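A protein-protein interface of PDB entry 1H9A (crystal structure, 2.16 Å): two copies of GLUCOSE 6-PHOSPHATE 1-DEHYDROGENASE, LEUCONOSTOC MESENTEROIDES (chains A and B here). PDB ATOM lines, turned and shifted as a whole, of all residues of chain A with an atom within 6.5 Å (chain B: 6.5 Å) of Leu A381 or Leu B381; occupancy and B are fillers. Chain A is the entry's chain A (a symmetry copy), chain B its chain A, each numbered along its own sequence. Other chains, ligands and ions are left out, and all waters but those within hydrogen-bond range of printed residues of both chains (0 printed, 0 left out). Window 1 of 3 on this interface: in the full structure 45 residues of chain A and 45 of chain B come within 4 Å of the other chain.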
ATOM      1  N   ILE A 197      -8.136 -12.357  22.092  1.00  0.00           N
ATOM      2  CA  ILE A 197      -7.970 -13.564  21.282  1.00  0.00           C
ATOM      3  C   ILE A 197      -6.701 -13.511  20.429  1.00  0.00           C
ATOM      4  O   ILE A 197      -6.126 -14.549  20.105  1.00  0.00           O
ATOM      5  CB  ILE A 197      -9.209 -13.880  20.405  1.00  0.00           C
ATOM      6  CG1 ILE A 197      -9.550 -12.696  19.504  1.00  0.00           C
ATOM      7  CG2 ILE A 197     -10.395 -14.272  21.291  1.00  0.00           C
ATOM      8  CD1 ILE A 197     -10.627 -13.009  18.499  1.00  0.00           C
ATOM      9  N   PHE A 198      -6.260 -12.303  20.079  1.00  0.00           N
ATOM     10  CA  PHE A 198      -5.031 -12.129  19.305  1.00  0.00           C
ATOM     11  C   PHE A 198      -3.843 -11.945  20.237  1.00  0.00           C
ATOM     12  O   PHE A 198      -2.787 -12.532  20.018  1.00  0.00           O
ATOM     13  CB  PHE A 198      -5.139 -10.954  18.342  1.00  0.00           C
ATOM     14  CG  PHE A 198      -5.976 -11.250  17.140  1.00  0.00           C
ATOM     15  CD1 PHE A 198      -5.966 -12.523  16.576  1.00  0.00           C
ATOM     16  CD2 PHE A 198      -6.795 -10.278  16.589  1.00  0.00           C
ATOM     17  CE1 PHE A 198      -6.763 -12.825  15.478  1.00  0.00           C
ATOM     18  CE2 PHE A 198      -7.599 -10.568  15.490  1.00  0.00           C
ATOM     19  CZ  PHE A 198      -7.584 -11.847  14.933  1.00  0.00           C
ATOM     20  N   PHE A 351      -0.776 -18.651  11.142  1.00  0.00           N
ATOM     21  CA  PHE A 351      -1.011 -19.407  12.366  1.00  0.00           C
ATOM     22  C   PHE A 351      -0.867 -20.900  12.071  1.00  0.00           C
ATOM     23  O   PHE A 351      -1.192 -21.357  10.974  1.00  0.00           O
ATOM     24  CB  PHE A 351      -2.408 -19.109  12.935  1.00  0.00           C
ATOM     25  CG  PHE A 351      -2.542 -17.724  13.514  1.00  0.00           C
ATOM     26  CD1 PHE A 351      -1.947 -17.407  14.736  1.00  0.00           C
ATOM     27  CD2 PHE A 351      -3.230 -16.729  12.825  1.00  0.00           C
ATOM     28  CE1 PHE A 351      -2.031 -16.120  15.258  1.00  0.00           C
ATOM     29  CE2 PHE A 351      -3.319 -15.436  13.340  1.00  0.00           C
ATOM     30  CZ  PHE A 351      -2.717 -15.130  14.557  1.00  0.00           C
ATOM     31  N   ALA A 367      -4.544 -20.632   9.398  1.00  0.00           N
ATOM     32  CA  ALA A 367      -5.309 -19.387   9.394  1.00  0.00           C
ATOM     33  C   ALA A 367      -4.284 -18.277   9.172  1.00  0.00           C
ATOM     34  O   ALA A 367      -3.133 -18.391   9.609  1.00  0.00           O
ATOM     35  CB  ALA A 367      -6.014 -19.188  10.726  1.00  0.00           C
ATOM     36  N   VAL A 368      -4.690 -17.200   8.513  1.00  0.00           N
ATOM     37  CA  VAL A 368      -3.768 -16.103   8.236  1.00  0.00           C
ATOM     38  C   VAL A 368      -4.355 -14.727   8.544  1.00  0.00           C
ATOM     39  O   VAL A 368      -5.472 -14.424   8.129  1.00  0.00           O
ATOM     40  CB  VAL A 368      -3.341 -16.120   6.741  1.00  0.00           C
ATOM     41  CG1 VAL A 368      -2.428 -14.947   6.431  1.00  0.00           C
ATOM     42  CG2 VAL A 368      -2.667 -17.440   6.393  1.00  0.00           C
ATOM     43  N   LEU A 369      -3.624 -13.910   9.296  1.00  0.00           N
ATOM     44  CA  LEU A 369      -4.070 -12.546   9.573  1.00  0.00           C
ATOM     45  C   LEU A 369      -3.198 -11.646   8.701  1.00  0.00           C
ATOM     46  O   LEU A 369      -1.974 -11.611   8.866  1.00  0.00           O
ATOM     47  CB  LEU A 369      -3.902 -12.169  11.048  1.00  0.00           C
ATOM     48  CG  LEU A 369      -4.131 -10.692  11.418  1.00  0.00           C
ATOM     49  CD1 LEU A 369      -5.518 -10.222  10.998  1.00  0.00           C
ATOM     50  CD2 LEU A 369      -3.932 -10.492  12.905  1.00  0.00           C
ATOM     51  N   SER A 370      -3.822 -10.973   7.741  1.00  0.00           N
ATOM     52  CA  SER A 370      -3.116 -10.080   6.830  1.00  0.00           C
ATOM     53  C   SER A 370      -3.479  -8.621   7.066  1.00  0.00           C
ATOM     54  O   SER A 370      -4.655  -8.274   7.194  1.00  0.00           O
ATOM     55  CB  SER A 370      -3.433 -10.429   5.371  1.00  0.00           C
ATOM     56  OG  SER A 370      -3.135 -11.780   5.076  1.00  0.00           O
ATOM     57  N   ILE A 379      -7.598  -5.227   6.173  1.00  0.00           N
ATOM     58  CA  ILE A 379      -7.310  -6.256   7.164  1.00  0.00           C
ATOM     59  C   ILE A 379      -8.133  -7.467   6.747  1.00  0.00           C
ATOM     60  O   ILE A 379      -9.335  -7.348   6.509  1.00  0.00           O
ATOM     61  CB  ILE A 379      -7.705  -5.816   8.598  1.00  0.00           C
ATOM     62  CG1 ILE A 379      -6.899  -4.585   9.012  1.00  0.00           C
ATOM     63  CG2 ILE A 379      -7.448  -6.950   9.583  1.00  0.00           C
ATOM     64  CD1 ILE A 379      -7.239  -4.054  10.374  1.00  0.00           C
ATOM     65  N   GLU A 380      -7.473  -8.611   6.602  1.00  0.00           N
ATOM     66  CA  GLU A 380      -8.137  -9.844   6.197  1.00  0.00           C
ATOM     67  C   GLU A 380      -7.776 -10.981   7.125  1.00  0.00           C
ATOM     68  O   GLU A 380      -6.645 -11.066   7.597  1.00  0.00           O
ATOM     69  CB  GLU A 380      -7.738 -10.230   4.777  1.00  0.00           C
ATOM     70  CG  GLU A 380      -8.173  -9.241   3.723  1.00  0.00           C
ATOM     71  CD  GLU A 380      -7.800  -9.693   2.328  1.00  0.00           C
ATOM     72  OE1 GLU A 380      -8.072 -10.872   1.992  1.00  0.00           O
ATOM     73  OE2 GLU A 380      -7.236  -8.869   1.572  1.00  0.00           O
ATOM     74  N   LEU A 381      -8.739 -11.851   7.394  1.00  0.00           N
ATOM     75  CA  LEU A 381      -8.506 -12.992   8.258  1.00  0.00           C
ATOM     76  C   LEU A 381      -9.011 -14.238   7.546  1.00  0.00           C
ATOM     77  O   LEU A 381     -10.218 -14.401   7.338  1.00  0.00           O
ATOM     78  CB  LEU A 381      -9.218 -12.813   9.600  1.00  0.00           C
ATOM     79  CG  LEU A 381      -9.043 -13.935  10.628  1.00  0.00           C
ATOM     80  CD1 LEU A 381      -7.593 -14.031  11.091  1.00  0.00           C
ATOM     81  CD2 LEU A 381      -9.966 -13.685  11.800  1.00  0.00           C
ATOM     82  N   LYS A 382      -8.069 -15.054   7.084  1.00  0.00           N
ATOM     83  CA  LYS A 382      -8.377 -16.295   6.394  1.00  0.00           C
ATOM     84  C   LYS A 382      -8.578 -17.361   7.465  1.00  0.00           C
ATOM     85  O   LYS A 382      -7.652 -17.684   8.207  1.00  0.00           O
ATOM     86  CB  LYS A 382      -7.224 -16.680   5.467  1.00  0.00           C
ATOM     87  CG  LYS A 382      -7.473 -17.936   4.649  1.00  0.00           C
ATOM     88  CD  LYS A 382      -6.265 -18.346   3.800  1.00  0.00           C
ATOM     89  CE  LYS A 382      -6.020 -17.400   2.614  1.00  0.00           C
ATOM     90  NZ  LYS A 382      -5.313 -16.130   2.978  1.00  0.00           N
ATOM     91  N   LEU A 383      -9.796 -17.887   7.554  1.00  0.00           N
ATOM     92  CA  LEU A 383     -10.133 -18.901   8.548  1.00  0.00           C
ATOM     93  C   LEU A 383     -10.617 -20.185   7.896  1.00  0.00           C
ATOM     94  O   LEU A 383     -10.995 -20.195   6.726  1.00  0.00           O
ATOM     95  CB  LEU A 383     -11.253 -18.395   9.457  1.00  0.00           C
ATOM     96  CG  LEU A 383     -11.011 -17.201  10.367  1.00  0.00           C
ATOM     97  CD1 LEU A 383     -12.320 -16.805  11.016  1.00  0.00           C
ATOM     98  CD2 LEU A 383      -9.973 -17.555  11.419  1.00  0.00           C
ATOM     99  N   ILE A 397     -12.019 -19.412   4.238  1.00  0.00           N
ATOM    100  CA  ILE A 397     -12.842 -18.288   3.815  1.00  0.00           C
ATOM    101  C   ILE A 397     -12.120 -17.046   4.303  1.00  0.00           C
ATOM    102  O   ILE A 397     -11.324 -17.124   5.243  1.00  0.00           O
ATOM    103  CB  ILE A 397     -14.275 -18.340   4.411  1.00  0.00           C
ATOM    104  CG1 ILE A 397     -14.225 -18.349   5.939  1.00  0.00           C
ATOM    105  CG2 ILE A 397     -15.041 -19.536   3.850  1.00  0.00           C
ATOM    106  CD1 ILE A 397     -15.567 -18.142   6.592  1.00  0.00           C
ATOM    107  N   ASP A 398     -12.389 -15.909   3.672  1.00  0.00           N
ATOM    108  CA  ASP A 398     -11.731 -14.664   4.039  1.00  0.00           C
ATOM    109  C   ASP A 398     -12.669 -13.618   4.597  1.00  0.00           C
ATOM    110  O   ASP A 398     -13.622 -13.217   3.928  1.00  0.00           O
ATOM    111  CB  ASP A 398     -11.014 -14.060   2.828  1.00  0.00           C
ATOM    112  CG  ASP A 398      -9.703 -14.750   2.517  1.00  0.00           C
ATOM    113  OD1 ASP A 398      -9.736 -15.887   1.996  1.00  0.00           O
ATOM    114  OD2 ASP A 398      -8.637 -14.148   2.787  1.00  0.00           O
ATOM    115  N   LEU A 399     -12.405 -13.190   5.828  1.00  0.00           N
ATOM    116  CA  LEU A 399     -13.196 -12.140   6.448  1.00  0.00           C
ATOM    117  C   LEU A 399     -12.386 -10.890   6.142  1.00  0.00           C
ATOM    118  O   LEU A 399     -11.195 -10.841   6.443  1.00  0.00           O
ATOM    119  CB  LEU A 399     -13.291 -12.323   7.961  1.00  0.00           C
ATOM    120  CG  LEU A 399     -13.739 -13.648   8.571  1.00  0.00           C
ATOM    121  CD1 LEU A 399     -14.237 -13.376   9.978  1.00  0.00           C
ATOM    122  CD2 LEU A 399     -14.826 -14.282   7.756  1.00  0.00           C
ATOM    123  N   GLY A 400     -13.006  -9.891   5.532  1.00  0.00           N
ATOM    124  CA  GLY A 400     -12.251  -8.704   5.207  1.00  0.00           C
ATOM    125  C   GLY A 400     -12.845  -7.389   5.643  1.00  0.00           C
ATOM    126  O   GLY A 400     -14.043  -7.276   5.896  1.00  0.00           O
ATOM    127  N   ILE B 197      -7.119 -20.453  17.299  1.00  0.00           N
ATOM    128  CA  ILE B 197      -7.344 -19.186  17.996  1.00  0.00           C
ATOM    129  C   ILE B 197      -8.758 -19.093  18.571  1.00  0.00           C
ATOM    130  O   ILE B 197      -8.980 -18.410  19.569  1.00  0.00           O
ATOM    131  CB  ILE B 197      -7.023 -17.948  17.119  1.00  0.00           C
ATOM    132  CG1 ILE B 197      -7.832 -17.976  15.825  1.00  0.00           C
ATOM    133  CG2 ILE B 197      -5.519 -17.875  16.840  1.00  0.00           C
ATOM    134  CD1 ILE B 197      -7.705 -16.712  15.019  1.00  0.00           C
ATOM    135  N   PHE B 198      -9.710 -19.789  17.947  1.00  0.00           N
ATOM    136  CA  PHE B 198     -11.088 -19.813  18.437  1.00  0.00           C
ATOM    137  C   PHE B 198     -11.292 -20.985  19.383  1.00  0.00           C
ATOM    138  O   PHE B 198     -11.913 -20.835  20.431  1.00  0.00           O
ATOM    139  CB  PHE B 198     -12.087 -19.877  17.287  1.00  0.00           C
ATOM    140  CG  PHE B 198     -12.252 -18.573  16.575  1.00  0.00           C
ATOM    141  CD1 PHE B 198     -12.188 -17.376  17.282  1.00  0.00           C
ATOM    142  CD2 PHE B 198     -12.441 -18.533  15.203  1.00  0.00           C
ATOM    143  CE1 PHE B 198     -12.306 -16.153  16.632  1.00  0.00           C
ATOM    144  CE2 PHE B 198     -12.561 -17.316  14.539  1.00  0.00           C
ATOM    145  CZ  PHE B 198     -12.492 -16.121  15.255  1.00  0.00           C
ATOM    146  N   PHE B 351     -17.033 -11.593  23.373  1.00  0.00           N
ATOM    147  CA  PHE B 351     -15.785 -11.854  24.082  1.00  0.00           C
ATOM    148  C   PHE B 351     -15.547 -10.745  25.107  1.00  0.00           C
ATOM    149  O   PHE B 351     -15.916  -9.592  24.880  1.00  0.00           O
ATOM    150  CB  PHE B 351     -14.605 -11.935  23.100  1.00  0.00           C
ATOM    151  CG  PHE B 351     -14.619 -13.171  22.238  1.00  0.00           C
ATOM    152  CD1 PHE B 351     -14.291 -14.415  22.778  1.00  0.00           C
ATOM    153  CD2 PHE B 351     -14.994 -13.099  20.899  1.00  0.00           C
ATOM    154  CE1 PHE B 351     -14.342 -15.567  21.999  1.00  0.00           C
ATOM    155  CE2 PHE B 351     -15.048 -14.248  20.110  1.00  0.00           C
ATOM    156  CZ  PHE B 351     -14.723 -15.485  20.662  1.00  0.00           C
ATOM    157  N   ALA B 367     -15.073  -7.798  21.668  1.00  0.00           N
ATOM    158  CA  ALA B 367     -15.023  -8.324  20.306  1.00  0.00           C
ATOM    159  C   ALA B 367     -16.230  -9.251  20.181  1.00  0.00           C
ATOM    160  O   ALA B 367     -16.638  -9.883  21.162  1.00  0.00           O
ATOM    161  CB  ALA B 367     -13.739  -9.104  20.080  1.00  0.00           C
ATOM    162  N   VAL B 368     -16.796  -9.352  18.986  1.00  0.00           N
ATOM    163  CA  VAL B 368     -17.968 -10.197  18.784  1.00  0.00           C
ATOM    164  C   VAL B 368     -17.870 -11.083  17.543  1.00  0.00           C
ATOM    165  O   VAL B 368     -17.537 -10.600  16.463  1.00  0.00           O
ATOM    166  CB  VAL B 368     -19.248  -9.325  18.652  1.00  0.00           C
ATOM    167  CG1 VAL B 368     -20.465 -10.194  18.383  1.00  0.00           C
ATOM    168  CG2 VAL B 368     -19.450  -8.479  19.902  1.00  0.00           C
ATOM    169  N   LEU B 369     -18.125 -12.378  17.700  1.00  0.00           N
ATOM    170  CA  LEU B 369     -18.135 -13.284  16.554  1.00  0.00           C
ATOM    171  C   LEU B 369     -19.607 -13.582  16.280  1.00  0.00           C
ATOM    172  O   LEU B 369     -20.299 -14.151  17.131  1.00  0.00           O
ATOM    173  CB  LEU B 369     -17.380 -14.587  16.838  1.00  0.00           C
ATOM    174  CG  LEU B 369     -17.508 -15.706  15.789  1.00  0.00           C
ATOM    175  CD1 LEU B 369     -17.063 -15.231  14.411  1.00  0.00           C
ATOM    176  CD2 LEU B 369     -16.704 -16.915  16.218  1.00  0.00           C
ATOM    177  N   SER B 370     -20.092 -13.141  15.124  1.00  0.00           N
ATOM    178  CA  SER B 370     -21.480 -13.349  14.732  1.00  0.00           C
ATOM    179  C   SER B 370     -21.605 -14.319  13.565  1.00  0.00           C
ATOM    180  O   SER B 370     -20.882 -14.210  12.573  1.00  0.00           O
ATOM    181  CB  SER B 370     -22.137 -12.022  14.333  1.00  0.00           C
ATOM    182  OG  SER B 370     -22.049 -11.060  15.365  1.00  0.00           O
ATOM    183  N   ILE B 379     -20.754 -14.431   8.223  1.00  0.00           N
ATOM    184  CA  ILE B 379     -19.904 -14.544   9.402  1.00  0.00           C
ATOM    185  C   ILE B 379     -19.224 -13.190   9.547  1.00  0.00           C
ATOM    186  O   ILE B 379     -18.650 -12.678   8.586  1.00  0.00           O
ATOM    187  CB  ILE B 379     -18.837 -15.659   9.252  1.00  0.00           C
ATOM    188  CG1 ILE B 379     -19.515 -17.019   9.081  1.00  0.00           C
ATOM    189  CG2 ILE B 379     -17.935 -15.689  10.479  1.00  0.00           C
ATOM    190  CD1 ILE B 379     -18.565 -18.163   8.885  1.00  0.00           C
ATOM    191  N   GLU B 380     -19.341 -12.591  10.727  1.00  0.00           N
ATOM    192  CA  GLU B 380     -18.747 -11.287  10.998  1.00  0.00           C
ATOM    193  C   GLU B 380     -17.950 -11.313  12.281  1.00  0.00           C
ATOM    194  O   GLU B 380     -18.331 -11.981  13.240  1.00  0.00           O
ATOM    195  CB  GLU B 380     -19.827 -10.217  11.118  1.00  0.00           C
ATOM    196  CG  GLU B 380     -20.611  -9.984   9.849  1.00  0.00           C
ATOM    197  CD  GLU B 380     -21.633  -8.880  10.004  1.00  0.00           C
ATOM    198  OE1 GLU B 380     -21.265  -7.797  10.524  1.00  0.00           O
ATOM    199  OE2 GLU B 380     -22.801  -9.096   9.608  1.00  0.00           O
ATOM    200  N   LEU B 381     -16.837 -10.594  12.298  1.00  0.00           N
ATOM    201  CA  LEU B 381     -15.999 -10.529  13.479  1.00  0.00           C
ATOM    202  C   LEU B 381     -15.711  -9.066  13.778  1.00  0.00           C
ATOM    203  O   LEU B 381     -15.013  -8.391  13.013  1.00  0.00           O
ATOM    204  CB  LEU B 381     -14.695 -11.301  13.266  1.00  0.00           C
ATOM    205  CG  LEU B 381     -13.715 -11.339  14.442  1.00  0.00           C
ATOM    206  CD1 LEU B 381     -14.306 -12.108  15.620  1.00  0.00           C
ATOM    207  CD2 LEU B 381     -12.417 -11.968  13.987  1.00  0.00           C
ATOM    208  N   LYS B 382     -16.341  -8.562  14.834  1.00  0.00           N
ATOM    209  CA  LYS B 382     -16.167  -7.187  15.269  1.00  0.00           C
ATOM    210  C   LYS B 382     -14.935  -7.156  16.165  1.00  0.00           C
ATOM    211  O   LYS B 382     -14.917  -7.781  17.224  1.00  0.00           O
ATOM    212  CB  LYS B 382     -17.401  -6.720  16.041  1.00  0.00           C
ATOM    213  CG  LYS B 382     -17.346  -5.269  16.488  1.00  0.00           C
ATOM    214  CD  LYS B 382     -18.554  -4.859  17.336  1.00  0.00           C
ATOM    215  CE  LYS B 382     -19.851  -4.750  16.517  1.00  0.00           C
ATOM    216  NZ  LYS B 382     -20.513  -6.065  16.238  1.00  0.00           N
ATOM    217  N   LEU B 383     -13.901  -6.446  15.725  1.00  0.00           N
ATOM    218  CA  LEU B 383     -12.651  -6.348  16.473  1.00  0.00           C
ATOM    219  C   LEU B 383     -12.322  -4.908  16.828  1.00  0.00           C
ATOM    220  O   LEU B 383     -12.865  -3.973  16.242  1.00  0.00           O
ATOM    221  CB  LEU B 383     -11.493  -6.892  15.636  1.00  0.00           C
ATOM    222  CG  LEU B 383     -11.459  -8.363  15.253  1.00  0.00           C
ATOM    223  CD1 LEU B 383     -10.317  -8.593  14.287  1.00  0.00           C
ATOM    224  CD2 LEU B 383     -11.293  -9.218  16.498  1.00  0.00           C
ATOM    225  N   ILE B 397     -14.162  -2.425  14.299  1.00  0.00           N
ATOM    226  CA  ILE B 397     -14.315  -2.568  12.859  1.00  0.00           C
ATOM    227  C   ILE B 397     -14.894  -3.955  12.645  1.00  0.00           C
ATOM    228  O   ILE B 397     -14.746  -4.825  13.507  1.00  0.00           O
ATOM    229  CB  ILE B 397     -12.969  -2.430  12.098  1.00  0.00           C
ATOM    230  CG1 ILE B 397     -11.965  -3.478  12.580  1.00  0.00           C
ATOM    231  CG2 ILE B 397     -12.428  -1.008  12.229  1.00  0.00           C
ATOM    232  CD1 ILE B 397     -10.731  -3.578  11.722  1.00  0.00           C
ATOM    233  N   ASP B 398     -15.551  -4.162  11.510  1.00  0.00           N
ATOM    234  CA  ASP B 398     -16.170  -5.446  11.215  1.00  0.00           C
ATOM    235  C   ASP B 398     -15.559  -6.164  10.033  1.00  0.00           C
ATOM    236  O   ASP B 398     -15.538  -5.629   8.924  1.00  0.00           O
ATOM    237  CB  ASP B 398     -17.667  -5.268  10.940  1.00  0.00           C
ATOM    238  CG  ASP B 398     -18.478  -5.079  12.203  1.00  0.00           C
ATOM    239  OD1 ASP B 398     -18.405  -3.983  12.802  1.00  0.00           O
ATOM    240  OD2 ASP B 398     -19.198  -6.028  12.594  1.00  0.00           O
ATOM    241  N   LEU B 399     -15.051  -7.367  10.277  1.00  0.00           N
ATOM    242  CA  LEU B 399     -14.494  -8.182   9.210  1.00  0.00           C
ATOM    243  C   LEU B 399     -15.668  -9.066   8.821  1.00  0.00           C
ATOM    244  O   LEU B 399     -16.252  -9.726   9.680  1.00  0.00           O
ATOM    245  CB  LEU B 399     -13.345  -9.058   9.708  1.00  0.00           C
ATOM    246  CG  LEU B 399     -12.173  -8.460  10.480  1.00  0.00           C
ATOM    247  CD1 LEU B 399     -10.998  -9.412  10.366  1.00  0.00           C
ATOM    248  CD2 LEU B 399     -11.796  -7.112   9.940  1.00  0.00           C
ATOM    249  N   GLY B 400     -16.035  -9.075   7.549  1.00  0.00           N
ATOM    250  CA  GLY B 400     -17.164  -9.886   7.160  1.00  0.00           C
ATOM    251  C   GLY B 400     -16.954 -10.817   5.992  1.00  0.00           C
ATOM    252  O   GLY B 400     -16.049 -10.635   5.179  1.00  0.00           O
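Of chain B, only Leu B381 and Leu B399 come within 4 Å of Leu A381. Of the printed residues of chain B, Leu A383 touches Phe B198. Leu B369 touches none of the printed residues of chain A. Printed residues of chain A within 4 Å of Ile B397: Ile A379 (3.8 Å). The nearest residue of chain B that does not touch Leu A381 is Ile B197 (4.8 Å).
Of the 16 printed residues of chain B, 8 touch a printed residue of chain A. Of the 16 printed residues of chain A, 8 touch a printed residue of chain B. Hydrophobic or aromatic side chains of chain A within 4 Å of the printed part of chain B: Phe A198, Ile A379, Leu A381, Leu A383, Ile A397 and Leu A399. Along chain A the printed residues that touch a printed residue of chain B span positions 198 to 400. Among the printed residues, 13 pairs touch across the chains. Among the printed residues, no Asp or Glu carboxylate lies within 4 Å of a Lys or Arg side-chain nitrogen of the other chain.
Among the printed residues, pairs that only touch across the chains: Phe A198 with Leu B383 (3.6 Å), Ile A379 with Ile B397 (3.8 Å), Leu A381 with Leu B381 (3.7 Å), Leu A381 with Leu B399 (3.9 Å), Leu A383 with Phe B198 (3.6 Å), Ile A397 with Ile B379 (3.8 Å), Asp A398 with Gly B400 (3.8 Å), Leu A399 with Leu B381 (3.9 Å), Leu A399 with Leu B399 (3.7 Å), Leu A399 with Gly B400 (3.5 Å), Gly A400 with Asp B398 (3.8 Å) and Gly A400 with Leu B399 (3.5 Å).
Phe A198 touches Leu B383, and with the chains exchanged Leu A383 touches Phe B198. Leu A381 touches Leu B399, and with the chains exchanged Leu A399 touches Leu B381. Asp A398 touches Gly B400, and with the chains exchanged Gly A400 touches Asp B398. Leu A399 touches Gly B400, and with the chains exchanged Gly A400 touches Leu B399.
The backbone NH (N) of Gly B400 is in hydrogen-bond range of the backbone carbonyl oxygen (O) of Gly A400 (3.2 Å).
N of Ile B397 lies within hydrogen-bond range of O of Leu B383 (2.8 Å). The backbone NH (N) of Ile A397 lies within hydrogen-bond range of the backbone carbonyl oxygen (O) of Leu A383 (2.8 Å). The side-chain amino group (NZ) of Lys A382 is in salt-bridge range of the side-chain carboxylate (OD2) of Asp A398 (3.9 Å). The side-chain amino group (NZ) of Lys B382 lies within salt-bridge range of the side-chain carboxylate (OD2) of Asp B398, 3.9 Å away. The backbone NH (N) of Leu B381 is in hydrogen-bond range of the backbone carbonyl oxygen (O) of Leu B399 (2.8 Å). N of Leu A381 is in hydrogen-bond range of O of Leu A399, 2.8 Å away.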
